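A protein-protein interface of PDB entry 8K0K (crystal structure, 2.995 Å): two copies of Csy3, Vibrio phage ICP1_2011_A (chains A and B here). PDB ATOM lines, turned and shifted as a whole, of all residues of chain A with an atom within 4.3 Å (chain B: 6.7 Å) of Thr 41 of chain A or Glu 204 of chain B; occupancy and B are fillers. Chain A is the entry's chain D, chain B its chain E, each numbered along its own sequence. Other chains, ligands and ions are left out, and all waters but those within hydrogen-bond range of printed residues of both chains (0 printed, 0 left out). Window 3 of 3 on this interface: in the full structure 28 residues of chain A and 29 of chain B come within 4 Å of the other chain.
Among the printed residues, merely in contact across the chains: Thr 41 of chain A with Glu 204 of chain B, Lys 42 of chain A with Glu 204 of chain B and Thr 43 of chain A with His 225 of chain B.
The side-chain hydroxyl (OG1) of Thr 41 of chain A is in hydrogen-bond range of the side-chain amide nitrogen (ND2) of Asn 66 of chain A (3.1 Å). The backbone carbonyl oxygen of Lys 42 of chain A is in hydrogen-bond range of the backbone NH of Val 65 of chain A, at 2.9 Å. N of His 225 of chain B sits at hydrogen-bond distance from OG of Ser 202 of chain B (2.8 Å). O of Gln 214 of chain B lies within hydrogen-bond range of N of Glu 204 of chain B (2.7 Å). The side-chain carboxylate (OE1) of Glu 204 of chain B is in hydrogen-bond range of a ring nitrogen (NE2) of His 225 of chain B (2.7 Å).
Thr 41 of chain A touches just one residue of chain B: Glu 204 (3.9 Å). Printed residues of chain B within 4 Å of Lys 42 of chain A: Glu 204 (3.5 Å) and Gln 227 (3.2 Å). Glu 204 of chain B touches just these residues of chain A: Thr 41 (3.9 Å), Lys 42 (3.5 Å) and Thr 43 (2.9 Å). Of the printed residues of chain A, Phe 205 of chain B touches Thr 43 (2.7 Å). The nearest residue of chain B that does not touch Thr 41 of chain A is Phe 216 of chain B (5.0 Å). The nearest printed residue of chain B that does not touch Thr 43 of chain A is Gln 203 of chain B (4.5 Å).
The side-chain amino group (NZ) of Lys 42 of chain A sits at hydrogen-bond distance from the side-chain amide oxygen (OE1) of Gln 227 of chain B (3.2 Å). The side-chain carboxylate of Glu 204 of chain B lies within hydrogen-bond range of the backbone NH of Thr 43 of chain A (2.9 Å). N of Phe 205 of chain B is in hydrogen-bond range of OG1 of Thr 43 of chain A, 2.7 Å away. O of Thr 43 of chain A sits at hydrogen-bond distance from NE2 of Gln 227 of chain B (3.0 Å).
No position is printed for both chains. Of the 7 pairs that touch across the chains among the printed residues, none has its exchanged pair printed and touching as well.
Of the 13 printed residues of chain B, 4 touch a printed residue of chain A. Hydrophobic or aromatic side chains of chain B within 4 Å of the printed part of chain A: Phe 205 and His 225. Of the 8 printed residues of chain A, 3 touch a printed residue of chain B. Among the printed residues, 7 pairs touch across the chains.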
ATOM      1  N   GLY A  40      -3.816  -5.382  -8.366  1.00  0.00           N
ATOM      2  CA  GLY A  40      -2.510  -5.872  -7.994  1.00  0.00           C
ATOM      3  C   GLY A  40      -1.680  -4.781  -7.335  1.00  0.00           C
ATOM      4  O   GLY A  40      -2.076  -3.611  -7.281  1.00  0.00           O
ATOM      5  N   THR A  41      -0.509  -5.180  -6.843  1.00  0.00           N
ATOM      6  CA  THR A  41       0.431  -4.275  -6.198  1.00  0.00           C
ATOM      7  C   THR A  41       1.769  -4.366  -6.915  1.00  0.00           C
ATOM      8  O   THR A  41       2.246  -5.466  -7.210  1.00  0.00           O
ATOM      9  CB  THR A  41       0.602  -4.614  -4.711  1.00  0.00           C
ATOM     10  OG1 THR A  41      -0.655  -4.474  -4.039  1.00  0.00           O
ATOM     11  CG2 THR A  41       1.607  -3.678  -4.059  1.00  0.00           C
ATOM     12  N   LYS A  42       2.369  -3.214  -7.204  1.00  0.00           N
ATOM     13  CA  LYS A  42       3.662  -3.194  -7.869  1.00  0.00           C
ATOM     14  C   LYS A  42       4.511  -2.064  -7.305  1.00  0.00           C
ATOM     15  O   LYS A  42       3.993  -1.070  -6.784  1.00  0.00           O
ATOM     16  CB  LYS A  42       3.518  -3.042  -9.393  1.00  0.00           C
ATOM     17  CG  LYS A  42       3.304  -1.614  -9.874  1.00  0.00           C
ATOM     18  CD  LYS A  42       3.038  -1.557 -11.372  1.00  0.00           C
ATOM     19  CE  LYS A  42       2.740  -0.131 -11.823  1.00  0.00           C
ATOM     20  NZ  LYS A  42       2.347  -0.042 -13.255  1.00  0.00           N
ATOM     21  N   THR A  43       5.827  -2.239  -7.405  1.00  0.00           N
ATOM     22  CA  THR A  43       6.769  -1.188  -7.057  1.00  0.00           C
ATOM     23  C   THR A  43       6.855  -0.178  -8.193  1.00  0.00           C
ATOM     24  O   THR A  43       6.750  -0.535  -9.369  1.00  0.00           O
ATOM     25  CB  THR A  43       8.151  -1.779  -6.783  1.00  0.00           C
ATOM     26  OG1 THR A  43       8.045  -2.806  -5.790  1.00  0.00           O
ATOM     27  CG2 THR A  43       9.111  -0.703  -6.299  1.00  0.00           C
ATOM     28  N   VAL A  65       2.286   0.779  -5.335  1.00  0.00           N
ATOM     29  CA  VAL A  65       0.984   1.273  -5.757  1.00  0.00           C
ATOM     30  C   VAL A  65       0.127   0.108  -6.233  1.00  0.00           C
ATOM     31  O   VAL A  65       0.627  -0.940  -6.650  1.00  0.00           O
ATOM     32  CB  VAL A  65       1.083   2.342  -6.876  1.00  0.00           C
ATOM     33  CG1 VAL A  65       1.952   3.510  -6.442  1.00  0.00           C
ATOM     34  CG2 VAL A  65       1.619   1.732  -8.146  1.00  0.00           C
ATOM     35  N   ASN A  66      -1.187   0.313  -6.160  1.00  0.00           N
ATOM     36  CA  ASN A  66      -2.136  -0.602  -6.768  1.00  0.00           C
ATOM     37  C   ASN A  66      -2.252  -0.320  -8.263  1.00  0.00           C
ATOM     38  O   ASN A  66      -2.073   0.812  -8.725  1.00  0.00           O
ATOM     39  CB  ASN A  66      -3.510  -0.487  -6.104  1.00  0.00           C
ATOM     40  CG  ASN A  66      -3.593  -1.233  -4.778  1.00  0.00           C
ATOM     41  OD1 ASN A  66      -4.463  -0.955  -3.952  1.00  0.00           O
ATOM     42  ND2 ASN A  66      -2.689  -2.180  -4.571  1.00  0.00           N
ATOM     43  N   PHE A  67      -2.543  -1.370  -9.021  1.00  0.00           N
ATOM     44  CA  PHE A  67      -2.641  -1.248 -10.466  1.00  0.00           C
ATOM     45  C   PHE A  67      -3.648  -2.264 -10.977  1.00  0.00           C
ATOM     46  O   PHE A  67      -3.921  -3.275 -10.326  1.00  0.00           O
ATOM     47  CB  PHE A  67      -1.270  -1.414 -11.143  1.00  0.00           C
ATOM     48  CG  PHE A  67      -0.772  -2.838 -11.220  1.00  0.00           C
ATOM     49  CD1 PHE A  67      -0.975  -3.598 -12.360  1.00  0.00           C
ATOM     50  CD2 PHE A  67      -0.054  -3.398 -10.176  1.00  0.00           C
ATOM     51  CE1 PHE A  67      -0.495  -4.900 -12.449  1.00  0.00           C
ATOM     52  CE2 PHE A  67       0.426  -4.703 -10.260  1.00  0.00           C
ATOM     53  CZ  PHE A  67       0.205  -5.449 -11.402  1.00  0.00           C
ATOM     54  N   LEU A 211       1.182   1.558   1.094  1.00  0.00           N
ATOM     55  CA  LEU A 211       0.781   1.867  -0.302  1.00  0.00           C
ATOM     56  C   LEU A 211       0.665   3.380  -0.493  1.00  0.00           C
ATOM     57  O   LEU A 211       0.032   4.023   0.344  1.00  0.00           O
ATOM     58  CB  LEU A 211      -0.541   1.157  -0.613  1.00  0.00           C
ATOM     59  CG  LEU A 211      -0.444  -0.329  -0.942  1.00  0.00           C
ATOM     60  CD1 LEU A 211      -1.803  -0.875  -1.342  1.00  0.00           C
ATOM     61  CD2 LEU A 211       0.562  -0.571  -2.051  1.00  0.00           C
ATOM     62  N   SER B 202      11.540  -6.898 -14.365  1.00  0.00           N
ATOM     63  CA  SER B 202      11.518  -5.764 -13.452  1.00  0.00           C
ATOM     64  C   SER B 202      11.687  -6.241 -12.016  1.00  0.00           C
ATOM     65  O   SER B 202      11.240  -7.328 -11.643  1.00  0.00           O
ATOM     66  CB  SER B 202      10.213  -4.982 -13.593  1.00  0.00           C
ATOM     67  OG  SER B 202      10.245  -4.154 -14.737  1.00  0.00           O
ATOM     68  N   GLN B 203      12.342  -5.416 -11.208  1.00  0.00           N
ATOM     69  CA  GLN B 203      12.613  -5.750  -9.820  1.00  0.00           C
ATOM     70  C   GLN B 203      11.676  -4.980  -8.899  1.00  0.00           C
ATOM     71  O   GLN B 203      11.277  -3.852  -9.192  1.00  0.00           O
ATOM     72  CB  GLN B 203      14.068  -5.452  -9.469  1.00  0.00           C
ATOM     73  CG  GLN B 203      15.028  -5.888 -10.551  1.00  0.00           C
ATOM     74  CD  GLN B 203      16.452  -5.986 -10.067  1.00  0.00           C
ATOM     75  OE1 GLN B 203      16.758  -5.638  -8.927  1.00  0.00           O
ATOM     76  NE2 GLN B 203      17.337  -6.471 -10.931  1.00  0.00           N
ATOM     77  N   GLU B 204      11.321  -5.608  -7.785  1.00  0.00           N
ATOM     78  CA  GLU B 204      10.364  -5.055  -6.844  1.00  0.00           C
ATOM     79  C   GLU B 204      11.066  -4.658  -5.554  1.00  0.00           C
ATOM     80  O   GLU B 204      12.163  -5.133  -5.244  1.00  0.00           O
ATOM     81  CB  GLU B 204       9.248  -6.063  -6.541  1.00  0.00           C
ATOM     82  CG  GLU B 204       8.359  -6.416  -7.727  1.00  0.00           C
ATOM     83  CD  GLU B 204       7.237  -5.417  -7.946  1.00  0.00           C
ATOM     84  OE1 GLU B 204       7.484  -4.373  -8.577  1.00  0.00           O
ATOM     85  OE2 GLU B 204       6.107  -5.672  -7.475  1.00  0.00           O
ATOM     86  N   PHE B 205      10.416  -3.773  -4.803  1.00  0.00           N
ATOM     87  CA  PHE B 205      10.904  -3.334  -3.500  1.00  0.00           C
ATOM     88  C   PHE B 205      10.214  -4.167  -2.432  1.00  0.00           C
ATOM     89  O   PHE B 205       9.006  -4.034  -2.215  1.00  0.00           O
ATOM     90  CB  PHE B 205      10.643  -1.846  -3.283  1.00  0.00           C
ATOM     91  CG  PHE B 205      11.009  -1.362  -1.908  1.00  0.00           C
ATOM     92  CD1 PHE B 205      12.268  -1.615  -1.380  1.00  0.00           C
ATOM     93  CD2 PHE B 205      10.103  -0.640  -1.147  1.00  0.00           C
ATOM     94  CE1 PHE B 205      12.609  -1.167  -0.119  1.00  0.00           C
ATOM     95  CE2 PHE B 205      10.439  -0.187   0.112  1.00  0.00           C
ATOM     96  CZ  PHE B 205      11.694  -0.450   0.626  1.00  0.00           C
ATOM     97  N   VAL B 206      10.985  -5.016  -1.766  1.00  0.00           N
ATOM     98  CA  VAL B 206      10.487  -5.881  -0.708  1.00  0.00           C
ATOM     99  C   VAL B 206      11.112  -5.390   0.594  1.00  0.00           C
ATOM    100  O   VAL B 206      12.266  -5.705   0.911  1.00  0.00           O
ATOM    101  CB  VAL B 206      10.805  -7.356  -0.987  1.00  0.00           C
ATOM    102  CG1 VAL B 206      12.232  -7.519  -1.521  1.00  0.00           C
ATOM    103  CG2 VAL B 206      10.568  -8.215   0.253  1.00  0.00           C
ATOM    104  N   SER B 212      15.513 -10.815  -0.502  1.00  0.00           N
ATOM    105  CA  SER B 212      16.320  -9.614  -0.677  1.00  0.00           C
ATOM    106  C   SER B 212      16.256  -9.064  -2.095  1.00  0.00           C
ATOM    107  O   SER B 212      16.365  -7.848  -2.285  1.00  0.00           O
ATOM    108  CB  SER B 212      17.778  -9.889  -0.292  1.00  0.00           C
ATOM    109  OG  SER B 212      18.241 -11.095  -0.860  1.00  0.00           O
ATOM    110  N   LYS B 213      16.088  -9.930  -3.089  1.00  0.00           N
ATOM    111  CA  LYS B 213      15.711  -9.544  -4.442  1.00  0.00           C
ATOM    112  C   LYS B 213      14.343 -10.132  -4.742  1.00  0.00           C
ATOM    113  O   LYS B 213      14.083 -11.300  -4.436  1.00  0.00           O
ATOM    114  CB  LYS B 213      16.719 -10.043  -5.484  1.00  0.00           C
ATOM    115  CG  LYS B 213      17.702  -8.998  -5.984  1.00  0.00           C
ATOM    116  CD  LYS B 213      18.617  -8.504  -4.873  1.00  0.00           C
ATOM    117  CE  LYS B 213      19.955  -8.004  -5.427  1.00  0.00           C
ATOM    118  NZ  LYS B 213      20.899  -9.115  -5.769  1.00  0.00           N
ATOM    119  N   GLN B 214      13.465  -9.330  -5.333  1.00  0.00           N
ATOM    120  CA  GLN B 214      12.146  -9.803  -5.731  1.00  0.00           C
ATOM    121  C   GLN B 214      11.871  -9.343  -7.154  1.00  0.00           C
ATOM    122  O   GLN B 214      12.007  -8.154  -7.462  1.00  0.00           O
ATOM    123  CB  GLN B 214      11.066  -9.298  -4.773  1.00  0.00           C
ATOM    124  CG  GLN B 214       9.665  -9.763  -5.116  1.00  0.00           C
ATOM    125  CD  GLN B 214       8.644  -9.360  -4.068  1.00  0.00           C
ATOM    126  OE1 GLN B 214       8.990  -9.088  -2.918  1.00  0.00           O
ATOM    127  NE2 GLN B 214       7.375  -9.319  -4.466  1.00  0.00           N
ATOM    128  N   LEU B 215      11.495 -10.285  -8.018  1.00  0.00           N
ATOM    129  CA  LEU B 215      11.265 -10.010  -9.428  1.00  0.00           C
ATOM    130  C   LEU B 215       9.777  -9.862  -9.717  1.00  0.00           C
ATOM    131  O   LEU B 215       8.942 -10.544  -9.116  1.00  0.00           O
ATOM    132  CB  LEU B 215      11.864 -11.115 -10.296  1.00  0.00           C
ATOM    133  CG  LEU B 215      13.389 -11.052 -10.386  1.00  0.00           C
ATOM    134  CD1 LEU B 215      13.944 -12.239 -11.148  1.00  0.00           C
ATOM    135  CD2 LEU B 215      13.817  -9.750 -11.040  1.00  0.00           C
ATOM    136  N   PHE B 216       9.457  -8.963 -10.645  1.00  0.00           N
ATOM    137  CA  PHE B 216       8.071  -8.679 -10.993  1.00  0.00           C
ATOM    138  C   PHE B 216       7.437  -9.880 -11.683  1.00  0.00           C
ATOM    139  O   PHE B 216       8.025 -10.465 -12.597  1.00  0.00           O
ATOM    140  CB  PHE B 216       8.016  -7.452 -11.903  1.00  0.00           C
ATOM    141  CG  PHE B 216       6.626  -7.017 -12.271  1.00  0.00           C
ATOM    142  CD1 PHE B 216       5.650  -6.868 -11.305  1.00  0.00           C
ATOM    143  CD2 PHE B 216       6.310  -6.718 -13.584  1.00  0.00           C
ATOM    144  CE1 PHE B 216       4.378  -6.455 -11.648  1.00  0.00           C
ATOM    145  CE2 PHE B 216       5.040  -6.302 -13.927  1.00  0.00           C
ATOM    146  CZ  PHE B 216       4.075  -6.170 -12.956  1.00  0.00           C
ATOM    147  N   ASP B 217       6.230 -10.247 -11.253  1.00  0.00           N
ATOM    148  CA  ASP B 217       5.535 -11.386 -11.835  1.00  0.00           C
ATOM    149  C   ASP B 217       4.074 -11.041 -12.086  1.00  0.00           C
ATOM    150  O   ASP B 217       3.498 -10.170 -11.427  1.00  0.00           O
ATOM    151  CB  ASP B 217       5.614 -12.629 -10.935  1.00  0.00           C
ATOM    152  CG  ASP B 217       4.585 -12.604  -9.818  1.00  0.00           C
ATOM    153  OD1 ASP B 217       4.569 -11.626  -9.037  1.00  0.00           O
ATOM    154  OD2 ASP B 217       3.776 -13.555  -9.728  1.00  0.00           O
ATOM    155  N   HIS B 225       7.594  -3.973 -15.709  1.00  0.00           N
ATOM    156  CA  HIS B 225       6.647  -2.894 -15.464  1.00  0.00           C
ATOM    157  C   HIS B 225       6.450  -2.074 -16.728  1.00  0.00           C
ATOM    158  O   HIS B 225       7.403  -1.805 -17.464  1.00  0.00           O
ATOM    159  CB  HIS B 225       7.150  -1.981 -14.348  1.00  0.00           C
ATOM    160  CG  HIS B 225       7.339  -2.668 -13.035  1.00  0.00           C
ATOM    161  ND1 HIS B 225       8.399  -2.387 -12.201  1.00  0.00           N
ATOM    162  CD2 HIS B 225       6.596  -3.604 -12.400  1.00  0.00           C
ATOM    163  CE1 HIS B 225       8.309  -3.130 -11.114  1.00  0.00           C
ATOM    164  NE2 HIS B 225       7.223  -3.875 -11.208  1.00  0.00           N
ATOM    165  N   GLN B 227       5.957   0.995 -16.764  1.00  0.00           N
ATOM    166  CA  GLN B 227       6.692   2.242 -16.597  1.00  0.00           C
ATOM    167  C   GLN B 227       8.155   2.100 -17.006  1.00  0.00           C
ATOM    168  O   GLN B 227       8.760   3.078 -17.453  1.00  0.00           O
ATOM    169  CB  GLN B 227       6.579   2.748 -15.157  1.00  0.00           C
ATOM    170  CG  GLN B 227       7.380   1.976 -14.142  1.00  0.00           C
ATOM    171  CD  GLN B 227       6.508   1.196 -13.183  1.00  0.00           C
ATOM    172  OE1 GLN B 227       5.387   0.807 -13.516  1.00  0.00           O
ATOM    173  NE2 GLN B 227       7.017   0.966 -11.980  1.00  0.00           N
